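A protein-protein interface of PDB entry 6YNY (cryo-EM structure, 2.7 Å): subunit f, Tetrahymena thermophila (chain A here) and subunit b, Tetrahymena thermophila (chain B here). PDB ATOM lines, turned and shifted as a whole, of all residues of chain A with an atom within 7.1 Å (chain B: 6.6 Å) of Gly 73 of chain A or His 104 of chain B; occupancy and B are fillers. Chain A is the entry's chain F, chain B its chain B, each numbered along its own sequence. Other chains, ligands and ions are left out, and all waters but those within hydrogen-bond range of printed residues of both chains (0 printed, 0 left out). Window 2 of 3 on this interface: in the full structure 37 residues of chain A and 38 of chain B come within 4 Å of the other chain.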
ATOM      1  N   ASP A  16      24.684 -24.202  13.312  1.00  0.00           N
ATOM      2  CA  ASP A  16      23.999 -23.892  12.067  1.00  0.00           C
ATOM      3  C   ASP A  16      24.718 -22.742  11.379  1.00  0.00           C
ATOM      4  O   ASP A  16      24.836 -21.649  11.944  1.00  0.00           O
ATOM      5  CB  ASP A  16      22.537 -23.545  12.326  1.00  0.00           C
ATOM      6  CG  ASP A  16      21.749 -23.356  11.046  1.00  0.00           C
ATOM      7  OD1 ASP A  16      22.145 -22.512  10.216  1.00  0.00           O
ATOM      8  OD2 ASP A  16      20.739 -24.064  10.860  1.00  0.00           O
ATOM      9  N   SER A  18      23.928 -21.406   8.308  1.00  0.00           N
ATOM     10  CA  SER A  18      23.081 -20.548   7.499  1.00  0.00           C
ATOM     11  C   SER A  18      22.741 -19.276   8.261  1.00  0.00           C
ATOM     12  O   SER A  18      22.654 -19.261   9.492  1.00  0.00           O
ATOM     13  CB  SER A  18      21.796 -21.274   7.102  1.00  0.00           C
ATOM     14  OG  SER A  18      20.935 -21.447   8.213  1.00  0.00           O
ATOM     15  N   ALA A  20      19.881 -17.589   7.434  1.00  0.00           N
ATOM     16  CA  ALA A  20      18.577 -17.424   6.810  1.00  0.00           C
ATOM     17  C   ALA A  20      17.755 -16.341   7.487  1.00  0.00           C
ATOM     18  O   ALA A  20      16.989 -15.636   6.821  1.00  0.00           O
ATOM     19  CB  ALA A  20      17.828 -18.752   6.841  1.00  0.00           C
ATOM     20  N   ASP A  21      17.892 -16.197   8.800  1.00  0.00           N
ATOM     21  CA  ASP A  21      17.088 -15.249   9.553  1.00  0.00           C
ATOM     22  C   ASP A  21      17.707 -13.861   9.610  1.00  0.00           C
ATOM     23  O   ASP A  21      17.069 -12.936  10.123  1.00  0.00           O
ATOM     24  CB  ASP A  21      16.856 -15.775  10.969  1.00  0.00           C
ATOM     25  CG  ASP A  21      16.110 -17.094  10.981  1.00  0.00           C
ATOM     26  OD1 ASP A  21      15.132 -17.231  10.217  1.00  0.00           O
ATOM     27  OD2 ASP A  21      16.505 -17.999  11.742  1.00  0.00           O
ATOM     28  N   THR A  28       9.916 -16.175   8.647  1.00  0.00           N
ATOM     29  CA  THR A  28       8.624 -16.838   8.593  1.00  0.00           C
ATOM     30  C   THR A  28       7.778 -16.464   9.800  1.00  0.00           C
ATOM     31  O   THR A  28       8.291 -16.268  10.906  1.00  0.00           O
ATOM     32  CB  THR A  28       8.797 -18.356   8.539  1.00  0.00           C
ATOM     33  OG1 THR A  28       7.530 -18.978   8.301  1.00  0.00           O
ATOM     34  CG2 THR A  28       9.365 -18.881   9.841  1.00  0.00           C
ATOM     35  N   TYR A  33       5.483 -24.473   7.980  1.00  0.00           N
ATOM     36  CA  TYR A  33       5.382 -25.791   8.598  1.00  0.00           C
ATOM     37  C   TYR A  33       4.459 -25.656   9.802  1.00  0.00           C
ATOM     38  O   TYR A  33       4.870 -25.171  10.860  1.00  0.00           O
ATOM     39  CB  TYR A  33       6.749 -26.326   8.999  1.00  0.00           C
ATOM     40  CG  TYR A  33       7.705 -26.511   7.849  1.00  0.00           C
ATOM     41  CD1 TYR A  33       8.573 -25.501   7.476  1.00  0.00           C
ATOM     42  CD2 TYR A  33       7.739 -27.696   7.135  1.00  0.00           C
ATOM     43  CE1 TYR A  33       9.444 -25.667   6.432  1.00  0.00           C
ATOM     44  CE2 TYR A  33       8.610 -27.868   6.090  1.00  0.00           C
ATOM     45  CZ  TYR A  33       9.460 -26.851   5.743  1.00  0.00           C
ATOM     46  OH  TYR A  33      10.327 -27.023   4.697  1.00  0.00           O
ATOM     47  N   PRO A  70       9.208 -18.688   1.357  1.00  0.00           N
ATOM     48  CA  PRO A  70       9.246 -19.943   2.102  1.00  0.00           C
ATOM     49  C   PRO A  70      10.176 -19.811   3.302  1.00  0.00           C
ATOM     50  O   PRO A  70      10.816 -18.784   3.516  1.00  0.00           O
ATOM     51  CB  PRO A  70       9.768 -20.934   1.066  1.00  0.00           C
ATOM     52  CG  PRO A  70      10.635 -20.129   0.209  1.00  0.00           C
ATOM     53  CD  PRO A  70       9.997 -18.777   0.117  1.00  0.00           C
ATOM     54  N   ASP A  71      10.244 -20.877   4.091  1.00  0.00           N
ATOM     55  CA  ASP A  71      11.086 -20.913   5.284  1.00  0.00           C
ATOM     56  C   ASP A  71      12.484 -21.357   4.876  1.00  0.00           C
ATOM     57  O   ASP A  71      12.782 -22.547   4.788  1.00  0.00           O
ATOM     58  CB  ASP A  71      10.488 -21.828   6.340  1.00  0.00           C
ATOM     59  CG  ASP A  71      11.208 -21.736   7.666  1.00  0.00           C
ATOM     60  OD1 ASP A  71      12.125 -20.899   7.787  1.00  0.00           O
ATOM     61  OD2 ASP A  71      10.856 -22.497   8.590  1.00  0.00           O
ATOM     62  N   ARG A  72      13.356 -20.380   4.624  1.00  0.00           N
ATOM     63  CA  ARG A  72      14.708 -20.683   4.177  1.00  0.00           C
ATOM     64  C   ARG A  72      15.515 -21.406   5.244  1.00  0.00           C
ATOM     65  O   ARG A  72      16.519 -22.047   4.917  1.00  0.00           O
ATOM     66  CB  ARG A  72      15.416 -19.393   3.759  1.00  0.00           C
ATOM     67  CG  ARG A  72      14.655 -18.596   2.718  1.00  0.00           C
ATOM     68  CD  ARG A  72      15.421 -17.368   2.245  1.00  0.00           C
ATOM     69  NE  ARG A  72      16.517 -17.704   1.338  1.00  0.00           N
ATOM     70  CZ  ARG A  72      17.780 -17.889   1.710  1.00  0.00           C
ATOM     71  NH1 ARG A  72      18.693 -18.188   0.798  1.00  0.00           N
ATOM     72  NH2 ARG A  72      18.137 -17.774   2.982  1.00  0.00           N
ATOM     73  N   GLY A  73      15.102 -21.319   6.509  1.00  0.00           N
ATOM     74  CA  GLY A  73      15.807 -21.994   7.581  1.00  0.00           C
ATOM     75  C   GLY A  73      15.708 -23.503   7.539  1.00  0.00           C
ATOM     76  O   GLY A  73      16.559 -24.183   8.116  1.00  0.00           O
ATOM     77  N   ASN A  74      14.686 -24.041   6.879  1.00  0.00           N
ATOM     78  CA  ASN A  74      14.501 -25.479   6.759  1.00  0.00           C
ATOM     79  C   ASN A  74      15.200 -26.065   5.543  1.00  0.00           C
ATOM     80  O   ASN A  74      15.016 -27.250   5.250  1.00  0.00           O
ATOM     81  CB  ASN A  74      13.013 -25.818   6.693  1.00  0.00           C
ATOM     82  CG  ASN A  74      12.456 -26.264   8.020  1.00  0.00           C
ATOM     83  OD1 ASN A  74      12.690 -27.387   8.459  1.00  0.00           O
ATOM     84  ND2 ASN A  74      11.695 -25.393   8.660  1.00  0.00           N
ATOM     85  N   LYS A  75      15.994 -25.273   4.834  1.00  0.00           N
ATOM     86  CA  LYS A  75      16.659 -25.770   3.641  1.00  0.00           C
ATOM     87  C   LYS A  75      17.722 -26.799   3.990  1.00  0.00           C
ATOM     88  O   LYS A  75      18.497 -26.628   4.934  1.00  0.00           O
ATOM     89  CB  LYS A  75      17.294 -24.620   2.870  1.00  0.00           C
ATOM     90  CG  LYS A  75      16.337 -23.843   2.010  1.00  0.00           C
ATOM     91  CD  LYS A  75      17.020 -22.649   1.399  1.00  0.00           C
ATOM     92  CE  LYS A  75      16.107 -21.905   0.468  1.00  0.00           C
ATOM     93  NZ  LYS A  75      15.819 -22.673  -0.758  1.00  0.00           N
ATOM     94  N   ARG A  76      17.750 -27.878   3.214  1.00  0.00           N
ATOM     95  CA  ARG A  76      18.786 -28.899   3.320  1.00  0.00           C
ATOM     96  C   ARG A  76      18.790 -29.547   4.701  1.00  0.00           C
ATOM     97  O   ARG A  76      19.840 -29.893   5.242  1.00  0.00           O
ATOM     98  CB  ARG A  76      20.153 -28.308   2.988  1.00  0.00           C
ATOM     99  CG  ARG A  76      20.238 -27.701   1.603  1.00  0.00           C
ATOM    100  CD  ARG A  76      21.538 -26.959   1.395  1.00  0.00           C
ATOM    101  NE  ARG A  76      21.657 -25.789   2.258  1.00  0.00           N
ATOM    102  CZ  ARG A  76      21.275 -24.560   1.927  1.00  0.00           C
ATOM    103  NH1 ARG A  76      20.740 -24.310   0.743  1.00  0.00           N
ATOM    104  NH2 ARG A  76      21.433 -23.573   2.792  1.00  0.00           N
ATOM    105  N   ARG A  77      17.601 -29.722   5.274  1.00  0.00           N
ATOM    106  CA  ARG A  77      17.495 -30.290   6.611  1.00  0.00           C
ATOM    107  C   ARG A  77      17.574 -31.811   6.586  1.00  0.00           C
ATOM    108  O   ARG A  77      18.124 -32.422   7.507  1.00  0.00           O
ATOM    109  CB  ARG A  77      16.190 -29.833   7.253  1.00  0.00           C
ATOM    110  CG  ARG A  77      16.057 -30.147   8.719  1.00  0.00           C
ATOM    111  CD  ARG A  77      14.771 -29.589   9.253  1.00  0.00           C
ATOM    112  NE  ARG A  77      14.563 -29.888  10.661  1.00  0.00           N
ATOM    113  CZ  ARG A  77      13.554 -29.415  11.380  1.00  0.00           C
ATOM    114  NH1 ARG A  77      12.661 -28.613  10.828  1.00  0.00           N
ATOM    115  NH2 ARG A  77      13.442 -29.739  12.653  1.00  0.00           N
ATOM    116  N   LYS A  80      21.209 -32.726   6.312  1.00  0.00           N
ATOM    117  CA  LYS A  80      21.948 -32.484   7.544  1.00  0.00           C
ATOM    118  C   LYS A  80      21.698 -33.571   8.580  1.00  0.00           C
ATOM    119  O   LYS A  80      22.606 -33.937   9.334  1.00  0.00           O
ATOM    120  CB  LYS A  80      21.574 -31.114   8.097  1.00  0.00           C
ATOM    121  CG  LYS A  80      22.125 -29.971   7.287  1.00  0.00           C
ATOM    122  CD  LYS A  80      21.562 -28.651   7.737  1.00  0.00           C
ATOM    123  CE  LYS A  80      22.149 -27.515   6.942  1.00  0.00           C
ATOM    124  NZ  LYS A  80      21.668 -26.204   7.415  1.00  0.00           N
ATOM    125  N   ASN A  81      20.475 -34.097   8.642  1.00  0.00           N
ATOM    126  CA  ASN A  81      20.207 -35.200   9.555  1.00  0.00           C
ATOM    127  C   ASN A  81      20.880 -36.482   9.092  1.00  0.00           C
ATOM    128  O   ASN A  81      21.310 -37.289   9.921  1.00  0.00           O
ATOM    129  CB  ASN A  81      18.702 -35.412   9.701  1.00  0.00           C
ATOM    130  CG  ASN A  81      18.072 -34.458  10.684  1.00  0.00           C
ATOM    131  OD1 ASN A  81      17.854 -34.799  11.843  1.00  0.00           O
ATOM    132  ND2 ASN A  81      17.778 -33.256  10.229  1.00  0.00           N
ATOM    133  N   ARG A  84      24.540 -36.400  10.202  1.00  0.00           N
ATOM    134  CA  ARG A  84      24.701 -36.668  11.626  1.00  0.00           C
ATOM    135  C   ARG A  84      24.496 -38.143  11.938  1.00  0.00           C
ATOM    136  O   ARG A  84      25.181 -38.704  12.799  1.00  0.00           O
ATOM    137  CB  ARG A  84      23.725 -35.820  12.427  1.00  0.00           C
ATOM    138  CG  ARG A  84      24.112 -34.377  12.534  1.00  0.00           C
ATOM    139  CD  ARG A  84      22.920 -33.526  12.858  1.00  0.00           C
ATOM    140  NE  ARG A  84      22.155 -34.044  13.981  1.00  0.00           N
ATOM    141  CZ  ARG A  84      20.969 -33.576  14.349  1.00  0.00           C
ATOM    142  NH1 ARG A  84      20.409 -32.580  13.682  1.00  0.00           N
ATOM    143  NH2 ARG A  84      20.338 -34.106  15.382  1.00  0.00           N
ATOM    144  N   VAL B 101      20.190 -31.071  20.426  1.00  0.00           N
ATOM    145  CA  VAL B 101      19.147 -30.064  20.550  1.00  0.00           C
ATOM    146  C   VAL B 101      18.795 -29.538  19.168  1.00  0.00           C
ATOM    147  O   VAL B 101      19.671 -29.111  18.408  1.00  0.00           O
ATOM    148  CB  VAL B 101      19.602 -28.929  21.479  1.00  0.00           C
ATOM    149  CG1 VAL B 101      18.564 -27.840  21.534  1.00  0.00           C
ATOM    150  CG2 VAL B 101      19.876 -29.466  22.861  1.00  0.00           C
ATOM    151  N   SER B 102      17.510 -29.579  18.840  1.00  0.00           N
ATOM    152  CA  SER B 102      17.028 -29.037  17.583  1.00  0.00           C
ATOM    153  C   SER B 102      16.766 -27.548  17.738  1.00  0.00           C
ATOM    154  O   SER B 102      16.005 -27.158  18.631  1.00  0.00           O
ATOM    155  CB  SER B 102      15.760 -29.741  17.146  1.00  0.00           C
ATOM    156  OG  SER B 102      15.238 -29.169  15.965  1.00  0.00           O
ATOM    157  N   PRO B 103      17.372 -26.687  16.918  1.00  0.00           N
ATOM    158  CA  PRO B 103      17.092 -25.253  17.005  1.00  0.00           C
ATOM    159  C   PRO B 103      15.857 -24.814  16.240  1.00  0.00           C
ATOM    160  O   PRO B 103      15.563 -23.615  16.211  1.00  0.00           O
ATOM    161  CB  PRO B 103      18.352 -24.640  16.396  1.00  0.00           C
ATOM    162  CG  PRO B 103      18.763 -25.620  15.382  1.00  0.00           C
ATOM    163  CD  PRO B 103      18.417 -26.971  15.921  1.00  0.00           C
ATOM    164  N   HIS B 104      15.132 -25.742  15.636  1.00  0.00           N
ATOM    165  CA  HIS B 104      14.058 -25.406  14.723  1.00  0.00           C
ATOM    166  C   HIS B 104      12.745 -25.164  15.454  1.00  0.00           C
ATOM    167  O   HIS B 104      12.587 -25.458  16.640  1.00  0.00           O
ATOM    168  CB  HIS B 104      13.873 -26.513  13.692  1.00  0.00           C
ATOM    169  CG  HIS B 104      15.003 -26.637  12.725  1.00  0.00           C
ATOM    170  ND1 HIS B 104      16.115 -27.411  12.971  1.00  0.00           N
ATOM    171  CD2 HIS B 104      15.193 -26.084  11.505  1.00  0.00           C
ATOM    172  CE1 HIS B 104      16.940 -27.331  11.944  1.00  0.00           C
ATOM    173  NE2 HIS B 104      16.404 -26.531  11.042  1.00  0.00           N
ATOM    174  N   TYR B 105      11.791 -24.617  14.707  1.00  0.00           N
ATOM    175  CA  TYR B 105      10.454 -24.365  15.214  1.00  0.00           C
ATOM    176  C   TYR B 105       9.550 -25.580  15.111  1.00  0.00           C
ATOM    177  O   TYR B 105       8.516 -25.624  15.784  1.00  0.00           O
ATOM    178  CB  TYR B 105       9.831 -23.208  14.443  1.00  0.00           C
ATOM    179  CG  TYR B 105      10.600 -21.917  14.542  1.00  0.00           C
ATOM    180  CD1 TYR B 105      11.168 -21.515  15.737  1.00  0.00           C
ATOM    181  CD2 TYR B 105      10.760 -21.101  13.438  1.00  0.00           C
ATOM    182  CE1 TYR B 105      11.865 -20.341  15.829  1.00  0.00           C
ATOM    183  CE2 TYR B 105      11.457 -19.926  13.523  1.00  0.00           C
ATOM    184  CZ  TYR B 105      12.011 -19.550  14.720  1.00  0.00           C
ATOM    185  OH  TYR B 105      12.708 -18.374  14.809  1.00  0.00           O
ATOM    186  N   GLU B 106       9.910 -26.558  14.288  1.00  0.00           N
ATOM    187  CA  GLU B 106       9.113 -27.759  14.116  1.00  0.00           C
ATOM    188  C   GLU B 106      10.027 -28.970  14.069  1.00  0.00           C
ATOM    189  O   GLU B 106      11.197 -28.872  13.694  1.00  0.00           O
ATOM    190  CB  GLU B 106       8.264 -27.701  12.842  1.00  0.00           C
ATOM    191  CG  GLU B 106       9.050 -27.417  11.572  1.00  0.00           C
ATOM    192  CD  GLU B 106       9.403 -25.957  11.408  1.00  0.00           C
ATOM    193  OE1 GLU B 106       8.525 -25.101  11.635  1.00  0.00           O
ATOM    194  OE2 GLU B 106      10.564 -25.661  11.057  1.00  0.00           O
ATOM    195  N   SER B 107       9.477 -30.113  14.458  1.00  0.00           N
ATOM    196  CA  SER B 107      10.241 -31.345  14.463  1.00  0.00           C
ATOM    197  C   SER B 107      10.557 -31.785  13.036  1.00  0.00           C
ATOM    198  O   SER B 107       9.875 -31.423  12.075  1.00  0.00           O
ATOM    199  CB  SER B 107       9.482 -32.436  15.213  1.00  0.00           C
ATOM    200  OG  SER B 107       8.097 -32.369  14.948  1.00  0.00           O
ATOM    201  N   PHE B 108      11.615 -32.585  12.913  1.00  0.00           N
ATOM    202  CA  PHE B 108      12.114 -32.961  11.595  1.00  0.00           C
ATOM    203  C   PHE B 108      11.146 -33.879  10.860  1.00  0.00           C
ATOM    204  O   PHE B 108      10.956 -33.740   9.647  1.00  0.00           O
ATOM    205  CB  PHE B 108      13.479 -33.623  11.737  1.00  0.00           C
ATOM    206  CG  PHE B 108      13.977 -34.260  10.483  1.00  0.00           C
ATOM    207  CD1 PHE B 108      14.192 -33.513   9.347  1.00  0.00           C
ATOM    208  CD2 PHE B 108      14.244 -35.610  10.446  1.00  0.00           C
ATOM    209  CE1 PHE B 108      14.651 -34.101   8.201  1.00  0.00           C
ATOM    210  CE2 PHE B 108      14.703 -36.201   9.303  1.00  0.00           C
ATOM    211  CZ  PHE B 108      14.908 -35.446   8.178  1.00  0.00           C
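Of the 17 printed residues of chain A, 5 touch a printed residue of chain B.
Hydrophobic or aromatic side chains of chain A within 4 Å of the printed part of chain B: Tyr 33.
Of the 8 printed residues of chain B, 5 touch a printed residue of chain A.
Hydrophobic or aromatic side chains of chain B that line the printed part of chain A: His 104 and Phe 108.
Along chain B the printed residues that touch a printed residue of chain A span positions 102 to 108.
OE2 of Glu 106 of chain B lies within salt-bridge range of NH1 of Arg 77 of chain A.
The side-chain carboxylate (OE2) of Glu 106 of chain B lies within hydrogen-bond range of the side-chain amide nitrogen (ND2) of Asn 74 of chain A, at 2.7 Å.
The backbone NH (N) of Phe 108 of chain B lies close to the guanidinium group (NH2) of Arg 77 of chain A.
Of chain B, only His 104 (3.8 Å) comes within 4 Å of Gly 73 of chain A.
Of chain A, only Gly 73 (3.8 Å) and Arg 77 (3.4 Å) come within 4 Å of His 104 of chain B.
Of the printed residues of chain B, Tyr 33 of chain A touches Glu 106.
Printed residues of chain A within 4 Å of Ser 107 of chain B: Arg 77.
Of the printed residues of chain A, Phe 108 of chain B touches Arg 77 (3.4 Å) and Asn 81 (3.7 Å).
Arg 84 of chain A touches none of the printed residues of chain B.
The nearest printed residue of chain B that does not touch Gly 73 of chain A is Glu 106 of chain B (6.6 Å).
The nearest printed residue of chain B that does not touch Asn 74 of chain A is His 104 of chain B (4.2 Å).
The guanidinium group of Arg 77 of chain A sits at hydrogen-bond distance from the side-chain amide oxygen of Asn 74 of chain A (2.7 Å).
OD2 of Asp 71 of chain A is in hydrogen-bond range of ND2 of Asn 74 of chain A, at 3.0 Å.
The side-chain hydroxyl (OG) of Ser 102 of chain B lies close to the backbone NH (N) of His 104 of chain B (3.4 Å).
ND2 of Asn 81 of chain A sits at hydrogen-bond distance from O of Arg 77 of chain A, at 2.9 Å.
The backbone NH of Gly 73 of chain A sits close to the side-chain carboxylate of Asp 71 of chain A.
Among the printed residues, merely in contact across the chains: Tyr 33 of chain A with Glu 106 of chain B (3.4 Å), Gly 73 of chain A with His 104 of chain B (3.8 Å), Arg 77 of chain A with Ser 102 of chain B (3.8 Å), Arg 77 of chain A with His 104 of chain B (3.4 Å), Arg 77 of chain A with Ser 107 of chain B (3.6 Å) and Asn 81 of chain A with Phe 108 of chain B (3.7 Å).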
